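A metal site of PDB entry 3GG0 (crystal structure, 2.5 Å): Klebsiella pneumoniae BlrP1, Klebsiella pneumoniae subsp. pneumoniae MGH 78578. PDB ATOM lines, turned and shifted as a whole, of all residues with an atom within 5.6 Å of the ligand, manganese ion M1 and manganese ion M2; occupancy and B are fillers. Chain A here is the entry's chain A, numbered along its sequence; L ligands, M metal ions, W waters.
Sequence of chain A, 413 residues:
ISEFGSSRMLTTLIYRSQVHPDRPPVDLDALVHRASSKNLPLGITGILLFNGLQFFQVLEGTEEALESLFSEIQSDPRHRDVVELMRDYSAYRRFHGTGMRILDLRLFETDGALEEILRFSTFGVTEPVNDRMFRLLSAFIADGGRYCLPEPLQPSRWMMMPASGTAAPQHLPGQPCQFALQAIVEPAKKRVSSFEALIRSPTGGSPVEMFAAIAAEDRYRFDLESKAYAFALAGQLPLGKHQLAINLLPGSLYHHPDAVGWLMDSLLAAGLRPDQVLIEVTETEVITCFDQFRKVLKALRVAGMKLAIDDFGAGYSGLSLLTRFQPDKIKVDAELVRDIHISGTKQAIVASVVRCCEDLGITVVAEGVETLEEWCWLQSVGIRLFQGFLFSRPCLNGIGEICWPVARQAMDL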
ATOM      1  N   PHE A 179      -3.693   6.864  15.140  1.00  0.00           N
ATOM      2  CA  PHE A 179      -3.804   6.248  16.449  1.00  0.00           C
ATOM      3  C   PHE A 179      -3.162   7.097  17.526  1.00  0.00           C
ATOM      4  O   PHE A 179      -2.161   7.778  17.289  1.00  0.00           O
ATOM      5  CB  PHE A 179      -3.191   4.852  16.434  1.00  0.00           C
ATOM      6  CG  PHE A 179      -4.040   3.821  15.745  1.00  0.00           C
ATOM      7  CD1 PHE A 179      -4.079   3.733  14.350  1.00  0.00           C
ATOM      8  CD2 PHE A 179      -4.835   2.945  16.484  1.00  0.00           C
ATOM      9  CE1 PHE A 179      -4.873   2.788  13.719  1.00  0.00           C
ATOM     10  CE2 PHE A 179      -5.622   1.991  15.863  1.00  0.00           C
ATOM     11  CZ  PHE A 179      -5.651   1.915  14.473  1.00  0.00           C
ATOM     12  N   GLN A 182      -1.522   4.931  24.543  1.00  0.00           N
ATOM     13  CA  GLN A 182      -1.512   5.040  25.992  1.00  0.00           C
ATOM     14  C   GLN A 182      -0.612   3.986  26.605  1.00  0.00           C
ATOM     15  O   GLN A 182      -0.685   2.806  26.249  1.00  0.00           O
ATOM     16  CB  GLN A 182      -2.929   4.921  26.556  1.00  0.00           C
ATOM     17  CG  GLN A 182      -3.013   5.251  28.049  1.00  0.00           C
ATOM     18  CD  GLN A 182      -4.431   5.228  28.574  1.00  0.00           C
ATOM     19  OE1 GLN A 182      -5.328   4.627  27.974  1.00  0.00           O
ATOM     20  NE2 GLN A 182      -4.649   5.870  29.712  1.00  0.00           N
ATOM     21  N   GLU A 196      -1.018   0.824  24.398  1.00  0.00           N
ATOM     22  CA  GLU A 196      -2.245   0.500  23.675  1.00  0.00           C
ATOM     23  C   GLU A 196      -2.495   1.513  22.572  1.00  0.00           C
ATOM     24  O   GLU A 196      -2.469   2.717  22.806  1.00  0.00           O
ATOM     25  CB  GLU A 196      -3.449   0.444  24.623  1.00  0.00           C
ATOM     26  CG  GLU A 196      -4.663  -0.288  24.008  1.00  0.00           C
ATOM     27  CD  GLU A 196      -5.928  -0.180  24.852  1.00  0.00           C
ATOM     28  OE1 GLU A 196      -5.846   0.191  26.048  1.00  0.00           O
ATOM     29  OE2 GLU A 196      -7.010  -0.472  24.305  1.00  0.00           O
ATOM     30  N   ALA A 197      -2.724   1.008  21.358  1.00  0.00           N
ATOM     31  CA  ALA A 197      -3.107   1.838  20.236  1.00  0.00           C
ATOM     32  C   ALA A 197      -4.610   2.065  20.238  1.00  0.00           C
ATOM     33  O   ALA A 197      -5.383   1.104  20.281  1.00  0.00           O
ATOM     34  CB  ALA A 197      -2.665   1.205  18.941  1.00  0.00           C
ATOM     35  N   LEU A 198      -5.017   3.326  20.189  1.00  0.00           N
ATOM     36  CA  LEU A 198      -6.430   3.693  20.210  1.00  0.00           C
ATOM     37  C   LEU A 198      -6.770   4.530  18.983  1.00  0.00           C
ATOM     38  O   LEU A 198      -6.216   5.614  18.782  1.00  0.00           O
ATOM     39  CB  LEU A 198      -6.758   4.474  21.481  1.00  0.00           C
ATOM     40  CG  LEU A 198      -6.473   3.782  22.817  1.00  0.00           C
ATOM     41  CD1 LEU A 198      -6.448   4.785  23.962  1.00  0.00           C
ATOM     42  CD2 LEU A 198      -7.468   2.674  23.080  1.00  0.00           C
ATOM     43  N   ILE A 199      -7.692   4.027  18.159  1.00  0.00           N
ATOM     44  CA  ILE A 199      -7.992   4.630  16.856  1.00  0.00           C
ATOM     45  C   ILE A 199      -8.573   6.052  16.964  1.00  0.00           C
ATOM     46  O   ILE A 199      -9.415   6.343  17.818  1.00  0.00           O
ATOM     47  CB  ILE A 199      -8.920   3.719  16.018  1.00  0.00           C
ATOM     48  CG1 ILE A 199      -8.847   4.104  14.534  1.00  0.00           C
ATOM     49  CG2 ILE A 199     -10.349   3.756  16.532  1.00  0.00           C
ATOM     50  CD1 ILE A 199      -9.476   3.086  13.604  1.00  0.00           C
ATOM     51  N   ARG A 200      -8.081   6.941  16.109  1.00  0.00           N
ATOM     52  CA  ARG A 200      -8.603   8.296  16.015  1.00  0.00           C
ATOM     53  C   ARG A 200      -8.969   8.637  14.583  1.00  0.00           C
ATOM     54  O   ARG A 200      -8.351   8.130  13.630  1.00  0.00           O
ATOM     55  CB  ARG A 200      -7.579   9.311  16.546  1.00  0.00           C
ATOM     56  CG  ARG A 200      -7.159   9.089  18.002  1.00  0.00           C
ATOM     57  CD  ARG A 200      -8.237   9.558  18.961  1.00  0.00           C
ATOM     58  NE  ARG A 200      -7.839   9.395  20.357  1.00  0.00           N
ATOM     59  CZ  ARG A 200      -8.070   8.295  21.066  1.00  0.00           C
ATOM     60  NH1 ARG A 200      -8.693   7.249  20.524  1.00  0.00           N
ATOM     61  NH2 ARG A 200      -7.676   8.231  22.338  1.00  0.00           N
ATOM     62  N   SER A 206     -12.732  10.956  18.036  1.00  0.00           N
ATOM     63  CA  SER A 206     -12.886   9.720  18.798  1.00  0.00           C
ATOM     64  C   SER A 206     -13.046   8.479  17.908  1.00  0.00           C
ATOM     65  O   SER A 206     -13.352   8.606  16.726  1.00  0.00           O
ATOM     66  CB  SER A 206     -14.089   9.841  19.745  1.00  0.00           C
ATOM     67  OG  SER A 206     -15.305   9.684  19.060  1.00  0.00           O
ATOM     68  N   PRO A 207     -12.809   7.280  18.476  1.00  0.00           N
ATOM     69  CA  PRO A 207     -13.130   6.003  17.816  1.00  0.00           C
ATOM     70  C   PRO A 207     -14.539   5.974  17.223  1.00  0.00           C
ATOM     71  O   PRO A 207     -14.724   5.487  16.098  1.00  0.00           O
ATOM     72  CB  PRO A 207     -13.019   4.990  18.964  1.00  0.00           C
ATOM     73  CG  PRO A 207     -11.990   5.572  19.858  1.00  0.00           C
ATOM     74  CD  PRO A 207     -12.162   7.067  19.785  1.00  0.00           C
ATOM     75  N   PHE A 211     -15.491   5.472  13.209  1.00  0.00           N
ATOM     76  CA  PHE A 211     -16.309   4.392  12.663  1.00  0.00           C
ATOM     77  C   PHE A 211     -17.642   4.883  12.091  1.00  0.00           C
ATOM     78  O   PHE A 211     -18.211   4.233  11.219  1.00  0.00           O
ATOM     79  CB  PHE A 211     -16.532   3.299  13.714  1.00  0.00           C
ATOM     80  CG  PHE A 211     -15.393   2.316  13.825  1.00  0.00           C
ATOM     81  CD1 PHE A 211     -15.227   1.306  12.884  1.00  0.00           C
ATOM     82  CD2 PHE A 211     -14.477   2.411  14.873  1.00  0.00           C
ATOM     83  CE1 PHE A 211     -14.178   0.413  12.982  1.00  0.00           C
ATOM     84  CE2 PHE A 211     -13.424   1.519  14.981  1.00  0.00           C
ATOM     85  CZ  PHE A 211     -13.273   0.516  14.035  1.00  0.00           C
ATOM     86  N   ASP A 223     -11.758  -1.932  10.543  1.00  0.00           N
ATOM     87  CA  ASP A 223     -11.170  -2.204  11.857  1.00  0.00           C
ATOM     88  C   ASP A 223      -9.893  -3.030  11.717  1.00  0.00           C
ATOM     89  O   ASP A 223      -8.880  -2.731  12.345  1.00  0.00           O
ATOM     90  CB  ASP A 223     -12.177  -2.930  12.760  1.00  0.00           C
ATOM     91  CG  ASP A 223     -11.651  -3.172  14.163  1.00  0.00           C
ATOM     92  OD1 ASP A 223     -10.798  -2.389  14.628  1.00  0.00           O
ATOM     93  OD2 ASP A 223     -12.095  -4.141  14.809  1.00  0.00           O
ATOM     94  N   SER A 226      -7.162  -0.896   9.511  1.00  0.00           N
ATOM     95  CA  SER A 226      -6.558   0.240  10.228  1.00  0.00           C
ATOM     96  C   SER A 226      -5.375  -0.152  11.103  1.00  0.00           C
ATOM     97  O   SER A 226      -4.515   0.672  11.379  1.00  0.00           O
ATOM     98  CB  SER A 226      -7.612   0.972  11.062  1.00  0.00           C
ATOM     99  OG  SER A 226      -8.204   0.111  12.020  1.00  0.00           O
ATOM    100  N   LYS A 227      -5.326  -1.417  11.503  1.00  0.00           N
ATOM    101  CA  LYS A 227      -4.247  -1.911  12.352  1.00  0.00           C
ATOM    102  C   LYS A 227      -2.875  -1.791  11.710  1.00  0.00           C
ATOM    103  O   LYS A 227      -1.866  -1.715  12.408  1.00  0.00           O
ATOM    104  CB  LYS A 227      -4.520  -3.373  12.756  1.00  0.00           C
ATOM    105  CG  LYS A 227      -5.694  -3.534  13.699  1.00  0.00           C
ATOM    106  CD  LYS A 227      -5.770  -2.375  14.669  1.00  0.00           C
ATOM    107  CE  LYS A 227      -6.948  -2.495  15.578  1.00  0.00           C
ATOM    108  NZ  LYS A 227      -8.182  -1.932  14.972  1.00  0.00           N
ATOM    109  N   ASN A 247      -6.939  -3.175  19.763  1.00  0.00           N
ATOM    110  CA  ASN A 247      -8.353  -3.523  19.908  1.00  0.00           C
ATOM    111  C   ASN A 247      -8.958  -4.006  18.596  1.00  0.00           C
ATOM    112  O   ASN A 247      -9.015  -3.266  17.618  1.00  0.00           O
ATOM    113  CB  ASN A 247      -9.156  -2.319  20.424  1.00  0.00           C
ATOM    114  CG  ASN A 247      -8.648  -1.792  21.750  1.00  0.00           C
ATOM    115  OD1 ASN A 247      -9.132  -2.190  22.818  1.00  0.00           O
ATOM    116  ND2 ASN A 247      -7.679  -0.878  21.684  1.00  0.00           N
ATOM    117  N   LEU A 248      -9.392  -5.251  18.542  1.00  0.00           N
ATOM    118  CA  LEU A 248     -10.162  -5.758  17.408  1.00  0.00           C
ATOM    119  C   LEU A 248     -11.463  -6.381  17.882  1.00  0.00           C
ATOM    120  O   LEU A 248     -11.471  -7.138  18.855  1.00  0.00           O
ATOM    121  CB  LEU A 248      -9.356  -6.780  16.608  1.00  0.00           C
ATOM    122  CG  LEU A 248      -8.326  -6.271  15.602  1.00  0.00           C
ATOM    123  CD1 LEU A 248      -7.540  -7.445  15.015  1.00  0.00           C
ATOM    124  CD2 LEU A 248      -8.983  -5.468  14.507  1.00  0.00           C
ATOM    125  N   LEU A 249     -12.552  -6.064  17.201  1.00  0.00           N
ATOM    126  CA  LEU A 249     -13.786  -6.818  17.342  1.00  0.00           C
ATOM    127  C   LEU A 249     -13.592  -8.201  16.729  1.00  0.00           C
ATOM    128  O   LEU A 249     -12.916  -8.333  15.705  1.00  0.00           O
ATOM    129  CB  LEU A 249     -14.954  -6.087  16.665  1.00  0.00           C
ATOM    130  CG  LEU A 249     -15.172  -4.628  17.067  1.00  0.00           C
ATOM    131  CD1 LEU A 249     -16.321  -4.001  16.281  1.00  0.00           C
ATOM    132  CD2 LEU A 249     -15.408  -4.488  18.571  1.00  0.00           C
ATOM    133  N   GLU A 280      -6.582  -7.118  21.797  1.00  0.00           N
ATOM    134  CA  GLU A 280      -7.584  -6.871  22.827  1.00  0.00           C
ATOM    135  C   GLU A 280      -8.985  -7.087  22.275  1.00  0.00           C
ATOM    136  O   GLU A 280      -9.438  -6.371  21.384  1.00  0.00           O
ATOM    137  CB  GLU A 280      -7.467  -5.447  23.354  1.00  0.00           C
ATOM    138  CG  GLU A 280      -6.233  -5.178  24.186  1.00  0.00           C
ATOM    139  CD  GLU A 280      -6.285  -3.843  24.886  1.00  0.00           C
ATOM    140  OE1 GLU A 280      -5.221  -3.364  25.340  1.00  0.00           O
ATOM    141  OE2 GLU A 280      -7.383  -3.266  25.002  1.00  0.00           O
ATOM    142  N   THR A 282     -13.122  -7.417  23.462  1.00  0.00           N
ATOM    143  CA  THR A 282     -14.051  -7.079  24.542  1.00  0.00           C
ATOM    144  C   THR A 282     -14.787  -8.302  25.064  1.00  0.00           C
ATOM    145  O   THR A 282     -15.227  -9.160  24.295  1.00  0.00           O
ATOM    146  CB  THR A 282     -15.075  -6.007  24.130  1.00  0.00           C
ATOM    147  OG1 THR A 282     -15.387  -6.153  22.741  1.00  0.00           O
ATOM    148  CG2 THR A 282     -14.523  -4.623  24.375  1.00  0.00           C
ATOM    149  N   ASP A 310     -10.319  -7.561  26.982  1.00  0.00           N
ATOM    150  CA  ASP A 310     -10.499  -6.173  27.341  1.00  0.00           C
ATOM    151  C   ASP A 310     -11.786  -5.973  28.122  1.00  0.00           C
ATOM    152  O   ASP A 310     -12.778  -6.671  27.891  1.00  0.00           O
ATOM    153  CB  ASP A 310     -10.498  -5.299  26.092  1.00  0.00           C
ATOM    154  CG  ASP A 310     -10.211  -3.838  26.408  1.00  0.00           C
ATOM    155  OD1 ASP A 310      -9.879  -3.519  27.571  1.00  0.00           O
ATOM    156  OD2 ASP A 310     -10.308  -3.019  25.472  1.00  0.00           O
ATOM    157  N   ASP A 311     -11.766  -5.025  29.056  1.00  0.00           N
ATOM    158  CA  ASP A 311     -12.957  -4.652  29.840  1.00  0.00           C
ATOM    159  C   ASP A 311     -13.590  -5.837  30.578  1.00  0.00           C
ATOM    160  O   ASP A 311     -14.813  -5.998  30.589  1.00  0.00           O
ATOM    161  CB  ASP A 311     -13.984  -3.934  28.956  1.00  0.00           C
ATOM    162  CG  ASP A 311     -13.451  -2.610  28.401  1.00  0.00           C
ATOM    163  OD1 ASP A 311     -12.435  -2.096  28.926  1.00  0.00           O
ATOM    164  OD2 ASP A 311     -14.057  -2.080  27.443  1.00  0.00           O
ATOM    165  N   LYS A 331      -7.758  -7.317  31.376  1.00  0.00           N
ATOM    166  CA  LYS A 331      -7.844  -5.902  31.738  1.00  0.00           C
ATOM    167  C   LYS A 331      -9.100  -5.632  32.534  1.00  0.00           C
ATOM    168  O   LYS A 331     -10.207  -5.640  32.000  1.00  0.00           O
ATOM    169  CB  LYS A 331      -7.784  -5.012  30.507  1.00  0.00           C
ATOM    170  CG  LYS A 331      -6.568  -5.247  29.616  1.00  0.00           C
ATOM    171  CD  LYS A 331      -6.571  -4.336  28.410  1.00  0.00           C
ATOM    172  CE  LYS A 331      -5.811  -3.071  28.687  1.00  0.00           C
ATOM    173  NZ  LYS A 331      -6.102  -2.022  27.674  1.00  0.00           N
ATOM    174  N   ARG A 338     -13.306   2.472  39.641  1.00  0.00           N
ATOM    175  CA  ARG A 338     -14.015   3.627  40.209  1.00  0.00           C
ATOM    176  C   ARG A 338     -14.410   3.362  41.631  1.00  0.00           C
ATOM    177  O   ARG A 338     -15.188   2.440  41.901  1.00  0.00           O
ATOM    178  CB  ARG A 338     -15.274   3.954  39.401  1.00  0.00           C
ATOM    179  CG  ARG A 338     -15.028   4.680  38.116  1.00  0.00           C
ATOM    180  CD  ARG A 338     -14.350   6.039  38.322  1.00  0.00           C
ATOM    181  NE  ARG A 338     -13.676   6.437  37.091  1.00  0.00           N
ATOM    182  CZ  ARG A 338     -12.433   6.098  36.770  1.00  0.00           C
ATOM    183  NH1 ARG A 338     -11.696   5.392  37.621  1.00  0.00           N
ATOM    184  NH2 ARG A 338     -11.924   6.467  35.608  1.00  0.00           N
ATOM    185  N   GLU A 367      -7.684  -0.747  34.767  1.00  0.00           N
ATOM    186  CA  GLU A 367      -7.960   0.294  33.782  1.00  0.00           C
ATOM    187  C   GLU A 367      -8.637   1.487  34.399  1.00  0.00           C
ATOM    188  O   GLU A 367      -9.296   1.374  35.421  1.00  0.00           O
ATOM    189  CB  GLU A 367      -8.855  -0.251  32.700  1.00  0.00           C
ATOM    190  CG  GLU A 367      -8.176  -0.589  31.430  1.00  0.00           C
ATOM    191  CD  GLU A 367      -9.149  -1.013  30.383  1.00  0.00           C
ATOM    192  OE1 GLU A 367      -9.303  -0.300  29.370  1.00  0.00           O
ATOM    193  OE2 GLU A 367      -9.817  -2.046  30.594  1.00  0.00           O
ATOM    194  N   GLY A 368      -8.504   2.640  33.737  1.00  0.00           N
ATOM    195  CA  GLY A 368      -9.210   3.845  34.138  1.00  0.00           C
ATOM    196  C   GLY A 368      -8.793   4.355  35.503  1.00  0.00           C
ATOM    197  O   GLY A 368      -9.585   4.991  36.194  1.00  0.00           O
ATOM    198  N   VAL A 369      -7.551   4.086  35.892  1.00  0.00           N
ATOM    199  CA  VAL A 369      -7.000   4.577  37.160  1.00  0.00           C
ATOM    200  C   VAL A 369      -6.729   6.083  37.100  1.00  0.00           C
ATOM    201  O   VAL A 369      -5.872   6.541  36.342  1.00  0.00           O
ATOM    202  CB  VAL A 369      -5.704   3.834  37.548  1.00  0.00           C
ATOM    203  CG1 VAL A 369      -5.243   4.262  38.932  1.00  0.00           C
ATOM    204  CG2 VAL A 369      -5.920   2.328  37.498  1.00  0.00           C
ATOM    205  N   GLU A 370      -7.467   6.843  37.901  1.00  0.00           N
ATOM    206  CA  GLU A 370      -7.432   8.304  37.811  1.00  0.00           C
ATOM    207  C   GLU A 370      -6.884   8.972  39.068  1.00  0.00           C
ATOM    208  O   GLU A 370      -6.455  10.127  39.021  1.00  0.00           O
ATOM    209  CB  GLU A 370      -8.829   8.847  37.521  1.00  0.00           C
ATOM    210  CG  GLU A 370      -9.303   8.626  36.095  1.00  0.00           C
ATOM    211  CD  GLU A 370     -10.723   9.127  35.882  1.00  0.00           C
ATOM    212  OE1 GLU A 370     -11.439   9.312  36.875  1.00  0.00           O
ATOM    213  OE2 GLU A 370     -11.112   9.313  34.708  1.00  0.00           O
ATOM    214  N   GLN A 387      -3.207   1.128  33.976  1.00  0.00           N
ATOM    215  CA  GLN A 387      -3.470   1.983  32.836  1.00  0.00           C
ATOM    216  C   GLN A 387      -4.499   3.035  33.216  1.00  0.00           C
ATOM    217  O   GLN A 387      -5.587   2.703  33.682  1.00  0.00           O
ATOM    218  CB  GLN A 387      -3.975   1.159  31.647  1.00  0.00           C
ATOM    219  CG  GLN A 387      -4.328   1.983  30.405  1.00  0.00           C
ATOM    220  CD  GLN A 387      -4.701   1.123  29.208  1.00  0.00           C
ATOM    221  OE1 GLN A 387      -4.855  -0.081  29.308  1.00  0.00           O
ATOM    222  NE2 GLN A 387      -4.853   1.750  28.060  1.00  0.00           N
ATOM    223  N   GLY A 388      -4.162   4.306  33.037  1.00  0.00           N
ATOM    224  CA  GLY A 388      -5.096   5.378  33.335  1.00  0.00           C
ATOM    225  C   GLY A 388      -4.552   6.778  33.203  1.00  0.00           C
ATOM    226  O   GLY A 388      -3.335   6.975  33.073  1.00  0.00           O
ATOM    227  N   PHE A 389      -5.455   7.758  33.246  1.00  0.00           N
ATOM    228  CA  PHE A 389      -5.098   9.169  33.081  1.00  0.00           C
ATOM    229  C   PHE A 389      -4.158   9.664  34.180  1.00  0.00           C
ATOM    230  O   PHE A 389      -3.434  10.640  33.982  1.00  0.00           O
ATOM    231  CB  PHE A 389      -6.357  10.040  33.059  1.00  0.00           C
ATOM    232  CG  PHE A 389      -7.183   9.896  31.815  1.00  0.00           C
ATOM    233  CD1 PHE A 389      -6.674   9.274  30.687  1.00  0.00           C
ATOM    234  CD2 PHE A 389      -8.478  10.404  31.767  1.00  0.00           C
ATOM    235  CE1 PHE A 389      -7.436   9.145  29.524  1.00  0.00           C
ATOM    236  CE2 PHE A 389      -9.246  10.294  30.605  1.00  0.00           C
ATOM    237  CZ  PHE A 389      -8.723   9.654  29.494  1.00  0.00           C
ATOM    238  N   LEU A 390      -4.180   8.987  35.337  1.00  0.00           N
ATOM    239  CA  LEU A 390      -3.267   9.298  36.427  1.00  0.00           C
ATOM    240  C   LEU A 390      -1.815   9.160  35.997  1.00  0.00           C
ATOM    241  O   LEU A 390      -0.992  10.025  36.296  1.00  0.00           O
ATOM    242  CB  LEU A 390      -3.542   8.401  37.627  1.00  0.00           C
ATOM    243  CG  LEU A 390      -2.667   8.642  38.866  1.00  0.00           C
ATOM    244  CD1 LEU A 390      -3.071   9.928  39.583  1.00  0.00           C
ATOM    245  CD2 LEU A 390      -2.724   7.455  39.813  1.00  0.00           C
ATOM    246  N   SER A 392      -0.748   8.227  32.542  1.00  0.00           N
ATOM    247  CA  SER A 392      -0.462   8.512  31.141  1.00  0.00           C
ATOM    248  C   SER A 392      -1.733   8.700  30.337  1.00  0.00           C
ATOM    249  O   SER A 392      -2.631   7.860  30.359  1.00  0.00           O
ATOM    250  CB  SER A 392       0.371   7.374  30.532  1.00  0.00           C
ATOM    251  OG  SER A 392       0.588   7.566  29.144  1.00  0.00           O
ATOM    252  N   PRO A 394      -3.638   9.207  26.535  1.00  0.00           N
ATOM    253  CA  PRO A 394      -3.526   8.954  25.111  1.00  0.00           C
ATOM    254  C   PRO A 394      -2.823  10.085  24.392  1.00  0.00           C
ATOM    255  O   PRO A 394      -3.167  11.258  24.583  1.00  0.00           O
ATOM    256  CB  PRO A 394      -4.982   8.874  24.660  1.00  0.00           C
ATOM    257  CG  PRO A 394      -5.697   8.343  25.830  1.00  0.00           C
ATOM    258  CD  PRO A 394      -4.986   8.892  27.040  1.00  0.00           C
HETATM  259  P1  LIG L   1     -10.913   0.608  25.486  1.00  0.00           P
HETATM  260  O1  LIG L   1      -9.880   0.159  24.490  1.00  0.00           O
HETATM  261  O2  LIG L   1     -11.539  -0.621  26.105  1.00  0.00           O
HETATM  262  O3  LIG L   1     -10.187   1.466  26.637  1.00  0.00           O
HETATM  263  C1  LIG L   1      -9.420   2.627  26.301  1.00  0.00           C
HETATM  264  C2  LIG L   1     -10.291   3.870  26.474  1.00  0.00           C
HETATM  265  O4  LIG L   1     -10.319   4.253  27.845  1.00  0.00           O
HETATM  266  C3  LIG L   1      -9.678   5.067  25.777  1.00  0.00           C
HETATM  267  O5  LIG L   1     -10.744   5.880  25.291  1.00  0.00           O
HETATM  268  C4  LIG L   1      -9.004   5.809  26.881  1.00  0.00           C
HETATM  269  O6  LIG L   1      -8.926   7.105  26.589  1.00  0.00           O
HETATM  270  C5  LIG L   1      -9.785   5.607  27.948  1.00  0.00           C
HETATM  271  N1  LIG L   1      -9.128   5.788  29.139  1.00  0.00           N
HETATM  272  C6  LIG L   1      -7.937   5.398  29.373  1.00  0.00           C
HETATM  273  N2  LIG L   1      -7.637   5.737  30.581  1.00  0.00           N
HETATM  274  C7  LIG L   1      -8.676   6.370  31.166  1.00  0.00           C
HETATM  275  C8  LIG L   1      -8.917   6.948  32.416  1.00  0.00           C
HETATM  276  O7  LIG L   1      -8.052   6.932  33.319  1.00  0.00           O
HETATM  277  N3  LIG L   1     -10.122   7.510  32.641  1.00  0.00           N
HETATM  278  C9  LIG L   1     -11.083   7.533  31.679  1.00  0.00           C
HETATM  279  N4  LIG L   1     -12.272   8.107  31.951  1.00  0.00           N
HETATM  280  N5  LIG L   1     -10.860   6.979  30.457  1.00  0.00           N
HETATM  281  C10 LIG L   1      -9.677   6.403  30.198  1.00  0.00           C
HETATM  282  P2  LIG L   1     -10.926   5.761  23.696  1.00  0.00           P
HETATM  283  O8  LIG L   1     -11.527   7.126  23.135  1.00  0.00           O
HETATM  284  O9  LIG L   1      -9.528   5.549  22.958  1.00  0.00           O
HETATM  285  O10 LIG L   1     -11.629   4.372  23.307  1.00  0.00           O
HETATM  286  C11 LIG L   1     -13.036   4.197  23.167  1.00  0.00           C
HETATM  287  C12 LIG L   1     -13.035   2.690  22.911  1.00  0.00           C
HETATM  288  O11 LIG L   1     -13.001   2.415  21.498  1.00  0.00           O
HETATM  289  C13 LIG L   1     -11.836   1.941  23.490  1.00  0.00           C
HETATM  290  O12 LIG L   1     -12.111   1.476  24.812  1.00  0.00           O
HETATM  291  C14 LIG L   1     -11.685   0.814  22.509  1.00  0.00           C
HETATM  292  O13 LIG L   1     -12.634  -0.081  22.739  1.00  0.00           O
HETATM  293  C15 LIG L   1     -11.972   1.423  21.373  1.00  0.00           C
HETATM  294  N6  LIG L   1     -11.116   1.344  20.306  1.00  0.00           N
HETATM  295  C16 LIG L   1      -9.998   2.059  20.289  1.00  0.00           C
HETATM  296  N7  LIG L   1      -9.367   1.690  19.149  1.00  0.00           N
HETATM  297  C17 LIG L   1     -10.109   0.718  18.542  1.00  0.00           C
HETATM  298  C18 LIG L   1      -9.929   0.004  17.370  1.00  0.00           C
HETATM  299  O14 LIG L   1      -8.920   0.190  16.666  1.00  0.00           O
HETATM  300  N8  LIG L   1     -10.857  -0.920  17.020  1.00  0.00           N
HETATM  301  C19 LIG L   1     -11.956  -1.135  17.785  1.00  0.00           C
HETATM  302  N9  LIG L   1     -12.862  -2.060  17.383  1.00  0.00           N
HETATM  303  N10 LIG L   1     -12.154  -0.435  18.933  1.00  0.00           N
HETATM  304  C20 LIG L   1     -11.231   0.485  19.317  1.00  0.00           C
HETATM  305 MN    MN M   1     -10.534  -1.308  28.122  1.00  0.00          MN
HETATM  306 MN    MN M   2      -8.637  -1.732  24.857  1.00  0.00          MN
HETATM  307  O   HOH W   1     -10.835   3.282  30.435  1.00  0.00           O
HETATM  308  O   HOH W   2      -8.381  -1.114  27.113  1.00  0.00           O
HETATM  309  O   HOH W   3     -12.407   9.726  22.540  1.00  0.00           O
HETATM  310  O   HOH W   4      -6.747  -0.078  18.201  1.00  0.00           O
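O of Asn 247 sits at hydrogen-bond distance from N8 of the ligand (3.0 Å).
The backbone NH of Phe 389 sits at hydrogen-bond distance from an oxygen (O7) of the ligand (2.7 Å).
The side-chain carboxylate of Asp 223 sits at hydrogen-bond distance from a nitrogen (N8) of the ligand, at 2.8 Å.
An oxygen (O14) of the ligand is in hydrogen-bond range of the side-chain amino group of Lys 227, 2.8 Å away.
A nitrogen (N3) of the ligand lies within hydrogen-bond range of the side-chain carboxylate (OE2) of Glu 370, 2.9 Å away.
N of Ile 199 sits at hydrogen-bond distance from N7 of the ligand (3.0 Å).
The side-chain amide nitrogen (NE2) of Gln 182 is in hydrogen-bond range of a nitrogen (N2) of the ligand.
O9 of the ligand lies within salt-bridge range of NH1 of Arg 200.
O of Glu 280 lies within hydrogen-bond range of N of Leu 248, at 3.1 Å.
The side-chain carboxylate (OE1) of Glu 196 lies within hydrogen-bond range of the side-chain amide nitrogen (NE2) of Gln 387 (2.7 Å).
The side-chain amide nitrogen of Asn 247 sits at hydrogen-bond distance from the backbone carbonyl oxygen of Ala 197, 3.3 Å away.
OD1 of Asp 223 is in salt-bridge range of NZ of Lys 227.
OG of Ser 226 is in hydrogen-bond range of O of Asp 223.
O of Ser 392 sits at hydrogen-bond distance from NE2 of Gln 182, at 2.9 Å.
N of Leu 390 is in hydrogen-bond range of O of Val 369.
The side-chain amino group (NZ) of Lys 331 is in hydrogen-bond range of the side-chain amide oxygen (OE1) of Gln 387, 2.8 Å away.
Residues that only touch the ligand: Phe 179, Leu 198, Pro 207, Leu 249, Arg 338, Gly 368, Val 369, Gly 388 and Pro 394.
Hydrophobic or aromatic side chains within 4 Å of the ligand: Phe 179, Leu 198, Ile 199, Pro 207, Leu 249, Phe 389 and Pro 394.
Within 4 Å of the ligand: Phe 179, Gln 182, Glu 196, Leu 198, Ile 199, Arg 200, Pro 207, Asp 223, Lys 227, Asn 247, Leu 249, Asp 310, Asp 311, Arg 338, Glu 367, Gly 368, Val 369, Glu 370, Gly 388, Phe 389 and Pro 394.
Within 4 Å of manganese ion M1: Asp 310, Asp 311 and Glu 367.
The nearest printed residue that does not touch manganese ion M1 is Lys 331 (4.5 Å).
Merely in contact with manganese ion M2: Lys 331.
Of the 32 residues printed, 5 come within 4 Å of manganese ion M2.
Manganese ion M1 is bound by OE1 of Glu 367.
OD1 of Asp 311 is bound to manganese ion M1 (2.2 Å).
O2 of the ligand is bound to manganese ion M1 (2.4 Å).
OD1 of Asp 310 binds manganese ion M1, at 2.4 Å.
Water W2 binds manganese ion M1 (2.4 Å).
The side-chain carboxylate (OE2) of Glu 367 is bound to manganese ion M1, 2.7 Å away.
Manganese ion M1 has six donor atoms within binding distance.
Manganese ion M2 is bound by OE2 of Glu 280 (2.0 Å), OE2 of Glu 196 (2.1 Å), OD1 of Asn 247 (2.1 Å), OD2 of Asp 310 (2.2 Å), O1 of the ligand (2.3 Å) and water W2 (2.4 Å).
Water W2 lies within hydrogen-bond range of NZ of Lys 331, OE1 of Glu 196 and O3 of the ligand.
Water W4 lies within hydrogen-bond range of O14 of the ligand (2.7 Å), O of Ala 197 (2.8 Å) and N of Asn 247 (3.5 Å).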
